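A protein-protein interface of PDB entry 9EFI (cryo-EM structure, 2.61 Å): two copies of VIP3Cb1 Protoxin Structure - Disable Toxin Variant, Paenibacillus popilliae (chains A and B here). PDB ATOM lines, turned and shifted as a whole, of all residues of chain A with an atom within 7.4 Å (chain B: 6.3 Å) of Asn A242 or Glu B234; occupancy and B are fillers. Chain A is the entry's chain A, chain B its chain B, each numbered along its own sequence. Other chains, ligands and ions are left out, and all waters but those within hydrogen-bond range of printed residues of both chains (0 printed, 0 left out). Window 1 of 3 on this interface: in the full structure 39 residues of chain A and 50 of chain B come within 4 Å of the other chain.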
ATOM      1  N   LYS A 237      12.759   1.800 -31.185  1.00  0.00           N
ATOM      2  CA  LYS A 237      13.714   1.475 -30.131  1.00  0.00           C
ATOM      3  C   LYS A 237      15.142   1.515 -30.655  1.00  0.00           C
ATOM      4  O   LYS A 237      16.050   1.998 -29.969  1.00  0.00           O
ATOM      5  CB  LYS A 237      13.402   0.102 -29.536  1.00  0.00           C
ATOM      6  CG  LYS A 237      12.113   0.039 -28.738  1.00  0.00           C
ATOM      7  CD  LYS A 237      11.930  -1.332 -28.109  1.00  0.00           C
ATOM      8  CE  LYS A 237      10.645  -1.407 -27.303  1.00  0.00           C
ATOM      9  NZ  LYS A 237       9.442  -1.219 -28.158  1.00  0.00           N
ATOM     10  N   SER A 238      15.361   1.003 -31.868  1.00  0.00           N
ATOM     11  CA  SER A 238      16.705   1.005 -32.435  1.00  0.00           C
ATOM     12  C   SER A 238      17.207   2.423 -32.685  1.00  0.00           C
ATOM     13  O   SER A 238      18.377   2.727 -32.430  1.00  0.00           O
ATOM     14  CB  SER A 238      16.731   0.193 -33.729  1.00  0.00           C
ATOM     15  OG  SER A 238      15.894   0.779 -34.710  1.00  0.00           O
ATOM     16  N   VAL A 239      16.340   3.304 -33.185  1.00  0.00           N
ATOM     17  CA  VAL A 239      16.810   4.639 -33.545  1.00  0.00           C
ATOM     18  C   VAL A 239      16.860   5.568 -32.335  1.00  0.00           C
ATOM     19  O   VAL A 239      17.658   6.512 -32.310  1.00  0.00           O
ATOM     20  CB  VAL A 239      15.947   5.239 -34.668  1.00  0.00           C
ATOM     21  CG1 VAL A 239      15.951   4.328 -35.883  1.00  0.00           C
ATOM     22  CG2 VAL A 239      14.532   5.490 -34.184  1.00  0.00           C
ATOM     23  N   THR A 240      16.029   5.334 -31.323  1.00  0.00           N
ATOM     24  CA  THR A 240      15.978   6.190 -30.146  1.00  0.00           C
ATOM     25  C   THR A 240      16.800   5.653 -28.984  1.00  0.00           C
ATOM     26  O   THR A 240      16.781   6.249 -27.904  1.00  0.00           O
ATOM     27  CB  THR A 240      14.527   6.384 -29.696  1.00  0.00           C
ATOM     28  OG1 THR A 240      13.937   5.111 -29.415  1.00  0.00           O
ATOM     29  CG2 THR A 240      13.725   7.079 -30.781  1.00  0.00           C
ATOM     30  N   LYS A 241      17.512   4.546 -29.175  1.00  0.00           N
ATOM     31  CA  LYS A 241      18.343   3.982 -28.118  1.00  0.00           C
ATOM     32  C   LYS A 241      19.484   4.945 -27.818  1.00  0.00           C
ATOM     33  O   LYS A 241      20.376   5.141 -28.648  1.00  0.00           O
ATOM     34  CB  LYS A 241      18.873   2.614 -28.535  1.00  0.00           C
ATOM     35  CG  LYS A 241      19.548   1.835 -27.419  1.00  0.00           C
ATOM     36  CD  LYS A 241      19.955   0.451 -27.894  1.00  0.00           C
ATOM     37  CE  LYS A 241      20.523  -0.384 -26.760  1.00  0.00           C
ATOM     38  NZ  LYS A 241      21.738   0.236 -26.163  1.00  0.00           N
ATOM     39  N   ASN A 242      19.451   5.555 -26.634  1.00  0.00           N
ATOM     40  CA  ASN A 242      20.467   6.526 -26.230  1.00  0.00           C
ATOM     41  C   ASN A 242      21.734   5.759 -25.865  1.00  0.00           C
ATOM     42  O   ASN A 242      22.047   5.516 -24.698  1.00  0.00           O
ATOM     43  CB  ASN A 242      19.964   7.375 -25.070  1.00  0.00           C
ATOM     44  CG  ASN A 242      20.794   8.625 -24.862  1.00  0.00           C
ATOM     45  OD1 ASN A 242      21.982   8.660 -25.179  1.00  0.00           O
ATOM     46  ND2 ASN A 242      20.166   9.663 -24.326  1.00  0.00           N
ATOM     47  N   ASP A 243      22.478   5.374 -26.898  1.00  0.00           N
ATOM     48  CA  ASP A 243      23.664   4.550 -26.732  1.00  0.00           C
ATOM     49  C   ASP A 243      24.752   5.048 -27.672  1.00  0.00           C
ATOM     50  O   ASP A 243      24.553   5.990 -28.446  1.00  0.00           O
ATOM     51  CB  ASP A 243      23.342   3.072 -26.984  1.00  0.00           C
ATOM     52  CG  ASP A 243      23.230   2.739 -28.458  1.00  0.00           C
ATOM     53  OD1 ASP A 243      22.612   3.523 -29.203  1.00  0.00           O
ATOM     54  OD2 ASP A 243      23.765   1.689 -28.872  1.00  0.00           O
ATOM     55  N   MET A 244      25.920   4.416 -27.592  1.00  0.00           N
ATOM     56  CA  MET A 244      27.004   4.726 -28.511  1.00  0.00           C
ATOM     57  C   MET A 244      26.627   4.297 -29.924  1.00  0.00           C
ATOM     58  O   MET A 244      25.830   3.376 -30.121  1.00  0.00           O
ATOM     59  CB  MET A 244      28.293   4.032 -28.069  1.00  0.00           C
ATOM     60  CG  MET A 244      29.540   4.492 -28.805  1.00  0.00           C
ATOM     61  SD  MET A 244      31.021   3.596 -28.308  1.00  0.00           S
ATOM     62  CE  MET A 244      30.594   1.933 -28.810  1.00  0.00           C
ATOM     63  N   SER A 246      24.643   5.513 -31.956  1.00  0.00           N
ATOM     64  CA  SER A 246      23.200   5.522 -32.127  1.00  0.00           C
ATOM     65  C   SER A 246      22.828   6.260 -33.408  1.00  0.00           C
ATOM     66  O   SER A 246      23.686   6.733 -34.159  1.00  0.00           O
ATOM     67  CB  SER A 246      22.526   6.166 -30.920  1.00  0.00           C
ATOM     68  OG  SER A 246      21.122   6.224 -31.094  1.00  0.00           O
ATOM     69  N   PHE A 247      21.524   6.364 -33.663  1.00  0.00           N
ATOM     70  CA  PHE A 247      21.065   7.162 -34.793  1.00  0.00           C
ATOM     71  C   PHE A 247      21.416   8.630 -34.596  1.00  0.00           C
ATOM     72  O   PHE A 247      21.790   9.320 -35.552  1.00  0.00           O
ATOM     73  CB  PHE A 247      19.560   6.984 -34.988  1.00  0.00           C
ATOM     74  CG  PHE A 247      19.009   7.743 -36.157  1.00  0.00           C
ATOM     75  CD1 PHE A 247      19.430   7.457 -37.444  1.00  0.00           C
ATOM     76  CD2 PHE A 247      18.066   8.737 -35.974  1.00  0.00           C
ATOM     77  CE1 PHE A 247      18.926   8.152 -38.521  1.00  0.00           C
ATOM     78  CE2 PHE A 247      17.557   9.433 -37.049  1.00  0.00           C
ATOM     79  CZ  PHE A 247      17.988   9.139 -38.324  1.00  0.00           C
ATOM     80  N   GLU A 248      21.304   9.124 -33.361  1.00  0.00           N
ATOM     81  CA  GLU A 248      21.713  10.494 -33.076  1.00  0.00           C
ATOM     82  C   GLU A 248      23.213  10.680 -33.269  1.00  0.00           C
ATOM     83  O   GLU A 248      23.652  11.755 -33.693  1.00  0.00           O
ATOM     84  CB  GLU A 248      21.299  10.878 -31.656  1.00  0.00           C
ATOM     85  CG  GLU A 248      21.629  12.310 -31.278  1.00  0.00           C
ATOM     86  CD  GLU A 248      21.110  12.685 -29.905  1.00  0.00           C
ATOM     87  OE1 GLU A 248      20.285  11.928 -29.352  1.00  0.00           O
ATOM     88  OE2 GLU A 248      21.528  13.738 -29.378  1.00  0.00           O
ATOM     89  N   ARG A 313      10.491   8.862 -31.120  1.00  0.00           N
ATOM     90  CA  ARG A 313      10.451   9.162 -29.693  1.00  0.00           C
ATOM     91  C   ARG A 313       9.017   9.279 -29.199  1.00  0.00           C
ATOM     92  O   ARG A 313       8.678   8.770 -28.124  1.00  0.00           O
ATOM     93  CB  ARG A 313      11.226  10.444 -29.396  1.00  0.00           C
ATOM     94  CG  ARG A 313      12.730  10.294 -29.478  1.00  0.00           C
ATOM     95  CD  ARG A 313      13.427  11.485 -28.852  1.00  0.00           C
ATOM     96  NE  ARG A 313      13.035  11.663 -27.459  1.00  0.00           N
ATOM     97  CZ  ARG A 313      13.635  11.075 -26.433  1.00  0.00           C
ATOM     98  NH1 ARG A 313      14.660  10.258 -26.607  1.00  0.00           N
ATOM     99  NH2 ARG A 313      13.195  11.315 -25.201  1.00  0.00           N
ATOM    100  N   LEU A 318       8.300   8.202 -25.108  1.00  0.00           N
ATOM    101  CA  LEU A 318       9.419   8.749 -24.358  1.00  0.00           C
ATOM    102  C   LEU A 318       9.206  10.239 -24.098  1.00  0.00           C
ATOM    103  O   LEU A 318       8.247  10.856 -24.572  1.00  0.00           O
ATOM    104  CB  LEU A 318      10.726   8.509 -25.108  1.00  0.00           C
ATOM    105  CG  LEU A 318      11.081   7.052 -25.403  1.00  0.00           C
ATOM    106  CD1 LEU A 318      12.350   6.968 -26.232  1.00  0.00           C
ATOM    107  CD2 LEU A 318      11.234   6.277 -24.107  1.00  0.00           C
ATOM    108  N   ILE A 321      11.692  15.820 -26.262  1.00  0.00           N
ATOM    109  CA  ILE A 321      12.797  16.766 -26.354  1.00  0.00           C
ATOM    110  C   ILE A 321      12.750  17.389 -27.740  1.00  0.00           C
ATOM    111  O   ILE A 321      12.736  16.676 -28.752  1.00  0.00           O
ATOM    112  CB  ILE A 321      14.152  16.098 -26.079  1.00  0.00           C
ATOM    113  CG1 ILE A 321      14.258  14.760 -26.816  1.00  0.00           C
ATOM    114  CG2 ILE A 321      14.355  15.903 -24.584  1.00  0.00           C
ATOM    115  CD1 ILE A 321      15.551  14.026 -26.550  1.00  0.00           C
ATOM    116  N   TYR A 323      13.991  18.889 -30.917  1.00  0.00           N
ATOM    117  CA  TYR A 323      15.189  18.954 -31.740  1.00  0.00           C
ATOM    118  C   TYR A 323      15.191  20.157 -32.672  1.00  0.00           C
ATOM    119  O   TYR A 323      16.009  20.208 -33.595  1.00  0.00           O
ATOM    120  CB  TYR A 323      15.344  17.667 -32.553  1.00  0.00           C
ATOM    121  CG  TYR A 323      15.721  16.462 -31.725  1.00  0.00           C
ATOM    122  CD1 TYR A 323      17.026  16.282 -31.288  1.00  0.00           C
ATOM    123  CD2 TYR A 323      14.776  15.504 -31.385  1.00  0.00           C
ATOM    124  CE1 TYR A 323      17.378  15.184 -30.532  1.00  0.00           C
ATOM    125  CE2 TYR A 323      15.121  14.401 -30.630  1.00  0.00           C
ATOM    126  CZ  TYR A 323      16.423  14.247 -30.206  1.00  0.00           C
ATOM    127  OH  TYR A 323      16.775  13.151 -29.453  1.00  0.00           O
ATOM    128  N   TYR B 195      31.589  12.212 -29.299  1.00  0.00           N
ATOM    129  CA  TYR B 195      30.156  12.073 -29.076  1.00  0.00           C
ATOM    130  C   TYR B 195      29.865  11.402 -27.743  1.00  0.00           C
ATOM    131  O   TYR B 195      28.936  11.800 -27.035  1.00  0.00           O
ATOM    132  CB  TYR B 195      29.508  11.289 -30.214  1.00  0.00           C
ATOM    133  CG  TYR B 195      28.047  10.990 -29.970  1.00  0.00           C
ATOM    134  CD1 TYR B 195      27.076  11.958 -30.183  1.00  0.00           C
ATOM    135  CD2 TYR B 195      27.639   9.742 -29.518  1.00  0.00           C
ATOM    136  CE1 TYR B 195      25.741  11.691 -29.958  1.00  0.00           C
ATOM    137  CE2 TYR B 195      26.307   9.467 -29.290  1.00  0.00           C
ATOM    138  CZ  TYR B 195      25.363  10.445 -29.511  1.00  0.00           C
ATOM    139  OH  TYR B 195      24.034  10.175 -29.286  1.00  0.00           O
ATOM    140  N   LYS B 199      27.755  13.228 -24.852  1.00  0.00           N
ATOM    141  CA  LYS B 199      26.501  12.625 -24.421  1.00  0.00           C
ATOM    142  C   LYS B 199      26.532  12.289 -22.937  1.00  0.00           C
ATOM    143  O   LYS B 199      25.538  12.490 -22.230  1.00  0.00           O
ATOM    144  CB  LYS B 199      26.208  11.375 -25.247  1.00  0.00           C
ATOM    145  CG  LYS B 199      24.734  11.037 -25.338  1.00  0.00           C
ATOM    146  CD  LYS B 199      23.990  12.095 -26.135  1.00  0.00           C
ATOM    147  CE  LYS B 199      22.492  11.862 -26.116  1.00  0.00           C
ATOM    148  NZ  LYS B 199      21.925  12.051 -24.753  1.00  0.00           N
ATOM    149  N   GLU B 202      26.156  15.526 -21.031  1.00  0.00           N
ATOM    150  CA  GLU B 202      24.779  16.004 -21.113  1.00  0.00           C
ATOM    151  C   GLU B 202      23.859  15.204 -20.199  1.00  0.00           C
ATOM    152  O   GLU B 202      23.031  15.774 -19.480  1.00  0.00           O
ATOM    153  CB  GLU B 202      24.294  15.934 -22.560  1.00  0.00           C
ATOM    154  CG  GLU B 202      22.799  16.122 -22.724  1.00  0.00           C
ATOM    155  CD  GLU B 202      22.342  15.889 -24.149  1.00  0.00           C
ATOM    156  OE1 GLU B 202      23.202  15.869 -25.054  1.00  0.00           O
ATOM    157  OE2 GLU B 202      21.123  15.721 -24.363  1.00  0.00           O
ATOM    158  N   LEU B 203      23.991  13.876 -20.211  1.00  0.00           N
ATOM    159  CA  LEU B 203      23.124  13.042 -19.385  1.00  0.00           C
ATOM    160  C   LEU B 203      23.395  13.255 -17.902  1.00  0.00           C
ATOM    161  O   LEU B 203      22.456  13.317 -17.098  1.00  0.00           O
ATOM    162  CB  LEU B 203      23.293  11.570 -19.761  1.00  0.00           C
ATOM    163  CG  LEU B 203      22.770  11.185 -21.145  1.00  0.00           C
ATOM    164  CD1 LEU B 203      22.921   9.694 -21.384  1.00  0.00           C
ATOM    165  CD2 LEU B 203      21.321  11.611 -21.302  1.00  0.00           C
ATOM    166  N   LEU B 229      18.202   8.441 -15.561  1.00  0.00           N
ATOM    167  CA  LEU B 229      19.056   7.316 -15.206  1.00  0.00           C
ATOM    168  C   LEU B 229      18.901   6.165 -16.185  1.00  0.00           C
ATOM    169  O   LEU B 229      19.869   5.451 -16.445  1.00  0.00           O
ATOM    170  CB  LEU B 229      18.750   6.847 -13.784  1.00  0.00           C
ATOM    171  CG  LEU B 229      19.704   7.333 -12.693  1.00  0.00           C
ATOM    172  CD1 LEU B 229      21.108   6.814 -12.954  1.00  0.00           C
ATOM    173  CD2 LEU B 229      19.702   8.851 -12.603  1.00  0.00           C
ATOM    174  N   THR B 230      17.701   5.961 -16.732  1.00  0.00           N
ATOM    175  CA  THR B 230      17.521   4.924 -17.743  1.00  0.00           C
ATOM    176  C   THR B 230      18.318   5.240 -19.004  1.00  0.00           C
ATOM    177  O   THR B 230      18.982   4.361 -19.569  1.00  0.00           O
ATOM    178  CB  THR B 230      16.038   4.763 -18.073  1.00  0.00           C
ATOM    179  OG1 THR B 230      15.320   4.400 -16.888  1.00  0.00           O
ATOM    180  CG2 THR B 230      15.843   3.686 -19.126  1.00  0.00           C
ATOM    181  N   GLU B 231      18.265   6.494 -19.460  1.00  0.00           N
ATOM    182  CA  GLU B 231      19.051   6.880 -20.630  1.00  0.00           C
ATOM    183  C   GLU B 231      20.547   6.745 -20.360  1.00  0.00           C
ATOM    184  O   GLU B 231      21.302   6.236 -21.202  1.00  0.00           O
ATOM    185  CB  GLU B 231      18.708   8.310 -21.046  1.00  0.00           C
ATOM    186  CG  GLU B 231      17.268   8.496 -21.486  1.00  0.00           C
ATOM    187  CD  GLU B 231      16.978   9.911 -21.943  1.00  0.00           C
ATOM    188  OE1 GLU B 231      17.896  10.757 -21.889  1.00  0.00           O
ATOM    189  OE2 GLU B 231      15.830  10.179 -22.357  1.00  0.00           O
ATOM    190  N   LEU B 232      20.991   7.187 -19.181  1.00  0.00           N
ATOM    191  CA  LEU B 232      22.400   7.051 -18.830  1.00  0.00           C
ATOM    192  C   LEU B 232      22.805   5.590 -18.704  1.00  0.00           C
ATOM    193  O   LEU B 232      23.940   5.232 -19.030  1.00  0.00           O
ATOM    194  CB  LEU B 232      22.690   7.803 -17.532  1.00  0.00           C
ATOM    195  CG  LEU B 232      24.162   7.940 -17.154  1.00  0.00           C
ATOM    196  CD1 LEU B 232      24.949   8.528 -18.311  1.00  0.00           C
ATOM    197  CD2 LEU B 232      24.307   8.803 -15.918  1.00  0.00           C
ATOM    198  N   THR B 233      21.894   4.733 -18.238  1.00  0.00           N
ATOM    199  CA  THR B 233      22.173   3.306 -18.151  1.00  0.00           C
ATOM    200  C   THR B 233      22.318   2.692 -19.535  1.00  0.00           C
ATOM    201  O   THR B 233      23.184   1.840 -19.751  1.00  0.00           O
ATOM    202  CB  THR B 233      21.064   2.603 -17.370  1.00  0.00           C
ATOM    203  OG1 THR B 233      20.917   3.223 -16.087  1.00  0.00           O
ATOM    204  CG2 THR B 233      21.394   1.134 -17.180  1.00  0.00           C
ATOM    205  N   GLU B 234      21.475   3.104 -20.483  1.00  0.00           N
ATOM    206  CA  GLU B 234      21.635   2.637 -21.858  1.00  0.00           C
ATOM    207  C   GLU B 234      22.989   3.057 -22.417  1.00  0.00           C
ATOM    208  O   GLU B 234      23.701   2.253 -23.038  1.00  0.00           O
ATOM    209  CB  GLU B 234      20.502   3.173 -22.734  1.00  0.00           C
ATOM    210  CG  GLU B 234      19.129   2.642 -22.376  1.00  0.00           C
ATOM    211  CD  GLU B 234      18.041   3.197 -23.276  1.00  0.00           C
ATOM    212  OE1 GLU B 234      18.350   4.063 -24.121  1.00  0.00           O
ATOM    213  OE2 GLU B 234      16.878   2.765 -23.138  1.00  0.00           O
ATOM    214  N   LEU B 235      23.367   4.319 -22.191  1.00  0.00           N
ATOM    215  CA  LEU B 235      24.662   4.792 -22.672  1.00  0.00           C
ATOM    216  C   LEU B 235      25.810   4.021 -22.029  1.00  0.00           C
ATOM    217  O   LEU B 235      26.767   3.635 -22.710  1.00  0.00           O
ATOM    218  CB  LEU B 235      24.809   6.289 -22.404  1.00  0.00           C
ATOM    219  CG  LEU B 235      26.146   6.904 -22.822  1.00  0.00           C
ATOM    220  CD1 LEU B 235      26.353   6.766 -24.321  1.00  0.00           C
ATOM    221  CD2 LEU B 235      26.226   8.358 -22.401  1.00  0.00           C
ATOM    222  N   ALA B 236      25.728   3.784 -20.719  1.00  0.00           N
ATOM    223  CA  ALA B 236      26.775   3.048 -20.019  1.00  0.00           C
ATOM    224  C   ALA B 236      26.861   1.608 -20.505  1.00  0.00           C
ATOM    225  O   ALA B 236      27.959   1.061 -20.653  1.00  0.00           O
ATOM    226  CB  ALA B 236      26.524   3.090 -18.514  1.00  0.00           C
ATOM    227  N   LYS B 237      25.713   0.975 -20.746  1.00  0.00           N
ATOM    228  CA  LYS B 237      25.707  -0.397 -21.234  1.00  0.00           C
ATOM    229  C   LYS B 237      26.330  -0.481 -22.618  1.00  0.00           C
ATOM    230  O   LYS B 237      27.031  -1.449 -22.933  1.00  0.00           O
ATOM    231  CB  LYS B 237      24.278  -0.937 -21.245  1.00  0.00           C
ATOM    232  CG  LYS B 237      24.184  -2.450 -21.211  1.00  0.00           C
ATOM    233  CD  LYS B 237      22.737  -2.901 -21.117  1.00  0.00           C
ATOM    234  CE  LYS B 237      22.030  -2.229 -19.952  1.00  0.00           C
ATOM    235  NZ  LYS B 237      22.711  -2.510 -18.659  1.00  0.00           N
ATOM    236  N   SER B 238      26.077   0.520 -23.463  1.00  0.00           N
ATOM    237  CA  SER B 238      26.726   0.543 -24.771  1.00  0.00           C
ATOM    238  C   SER B 238      28.228   0.768 -24.647  1.00  0.00           C
ATOM    239  O   SER B 238      29.015   0.136 -25.360  1.00  0.00           O
ATOM    240  CB  SER B 238      26.101   1.623 -25.647  1.00  0.00           C
ATOM    241  OG  SER B 238      26.596   1.549 -26.971  1.00  0.00           O
ATOM    242  N   VAL B 239      28.644   1.672 -23.759  1.00  0.00           N
ATOM    243  CA  VAL B 239      30.059   2.016 -23.657  1.00  0.00           C
ATOM    244  C   VAL B 239      30.862   0.851 -23.088  1.00  0.00           C
ATOM    245  O   VAL B 239      31.942   0.519 -23.594  1.00  0.00           O
ATOM    246  CB  VAL B 239      30.239   3.293 -22.818  1.00  0.00           C
ATOM    247  CG1 VAL B 239      31.699   3.495 -22.461  1.00  0.00           C
ATOM    248  CG2 VAL B 239      29.712   4.498 -23.576  1.00  0.00           C
ATOM    249  N   LEU B 316      27.041   0.702 -13.750  1.00  0.00           N
ATOM    250  CA  LEU B 316      26.387  -0.578 -13.981  1.00  0.00           C
ATOM    251  C   LEU B 316      26.721  -1.618 -12.922  1.00  0.00           C
ATOM    252  O   LEU B 316      26.156  -2.715 -12.959  1.00  0.00           O
ATOM    253  CB  LEU B 316      26.765  -1.123 -15.358  1.00  0.00           C
ATOM    254  CG  LEU B 316      26.345  -0.278 -16.557  1.00  0.00           C
ATOM    255  CD1 LEU B 316      26.795  -0.950 -17.834  1.00  0.00           C
ATOM    256  CD2 LEU B 316      24.841  -0.074 -16.557  1.00  0.00           C
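Lys A241 touches Glu B234 (C to OE1, 3.97 Å). CD2 of Leu B203 touches ND2 of Asn A242, 3.8 Å away. OE1 of Glu B231 touches ND2 of Asn A242, at 3.5 Å. CE2 of Tyr B195 touches O of Asp A243, 3.98 Å away. CB of Glu A248 touches OH of Tyr B195, at 3.7 Å. Lys B199 touches Glu A248.
Of chain B, only Lys B199 (3.0 Å), Leu B203 (3.8 Å), Glu B231 (3.5 Å), Glu B234 (3.1 Å) and Leu B235 (3.1 Å) come within 4 Å of Asn A242. Of the printed residues of chain B, Glu A248 touches Tyr B195 and Lys B199. Of the printed residues of chain A, Lys B199 touches Asn A242 (3.0 Å) and Glu A248 (3.9 Å). Printed residues of chain A within 4 Å of Glu B231: Asn A242. Glu B234 touches just these residues of chain A: Lys A241 (3.97 Å) and Asn A242 (3.1 Å). Of the printed residues of chain A, Ser B238 touches Asp A243 (3.4 Å) and Met A244 (3.0 Å). The nearest residue of chain B that does not touch Asn A242 is Tyr B195 (4.8 Å). The nearest residue of chain A that does not touch Glu B234 is Asp A243 (4.05 Å).
N of Met A244 sits at hydrogen-bond distance from OG of Ser B238 (3.0 Å). OD2 of Asp A243 lies within hydrogen-bond range of OG of Ser B238 (3.4 Å). O of Asn A242 sits at hydrogen-bond distance from N of Leu B235 (3.1 Å). The side-chain amino group of Lys B199 sits close to the side-chain amide nitrogen of Asn A242. The backbone NH of Asn A242 is in hydrogen-bond range of the side-chain carboxylate of Glu B234 (3.1 Å).
3 positions are printed for both chains.
The side-chain carboxylate (OD2) of Asp A243 is in salt-bridge range of the side-chain amino group (NZ) of Lys A241. NZ of Lys B199 is in salt-bridge range of OE2 of Glu B202 (3.8 Å). The side-chain hydroxyl (OG) of Ser A246 sits at hydrogen-bond distance from the backbone carbonyl oxygen (O) of Lys A241 (2.8 Å).
Of the 16 printed residues of chain B, 7 touch a printed residue of chain A. Printed residues of chain B that touch a printed residue of chain A: Tyr B195, Lys B199, Leu B203, Glu B231, Glu B234, Leu B235 and Ser B238. Hydrophobic or aromatic side chains of chain B within 4 Å of the printed part of chain A: Tyr B195, Leu B203 and Leu B235. Of the 15 printed residues of chain A, 5 touch a printed residue of chain B. Hydrophobic or aromatic side chains of chain A that line the printed part of chain B: Met A244. Among the printed residues, 11 pairs touch across the chains.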
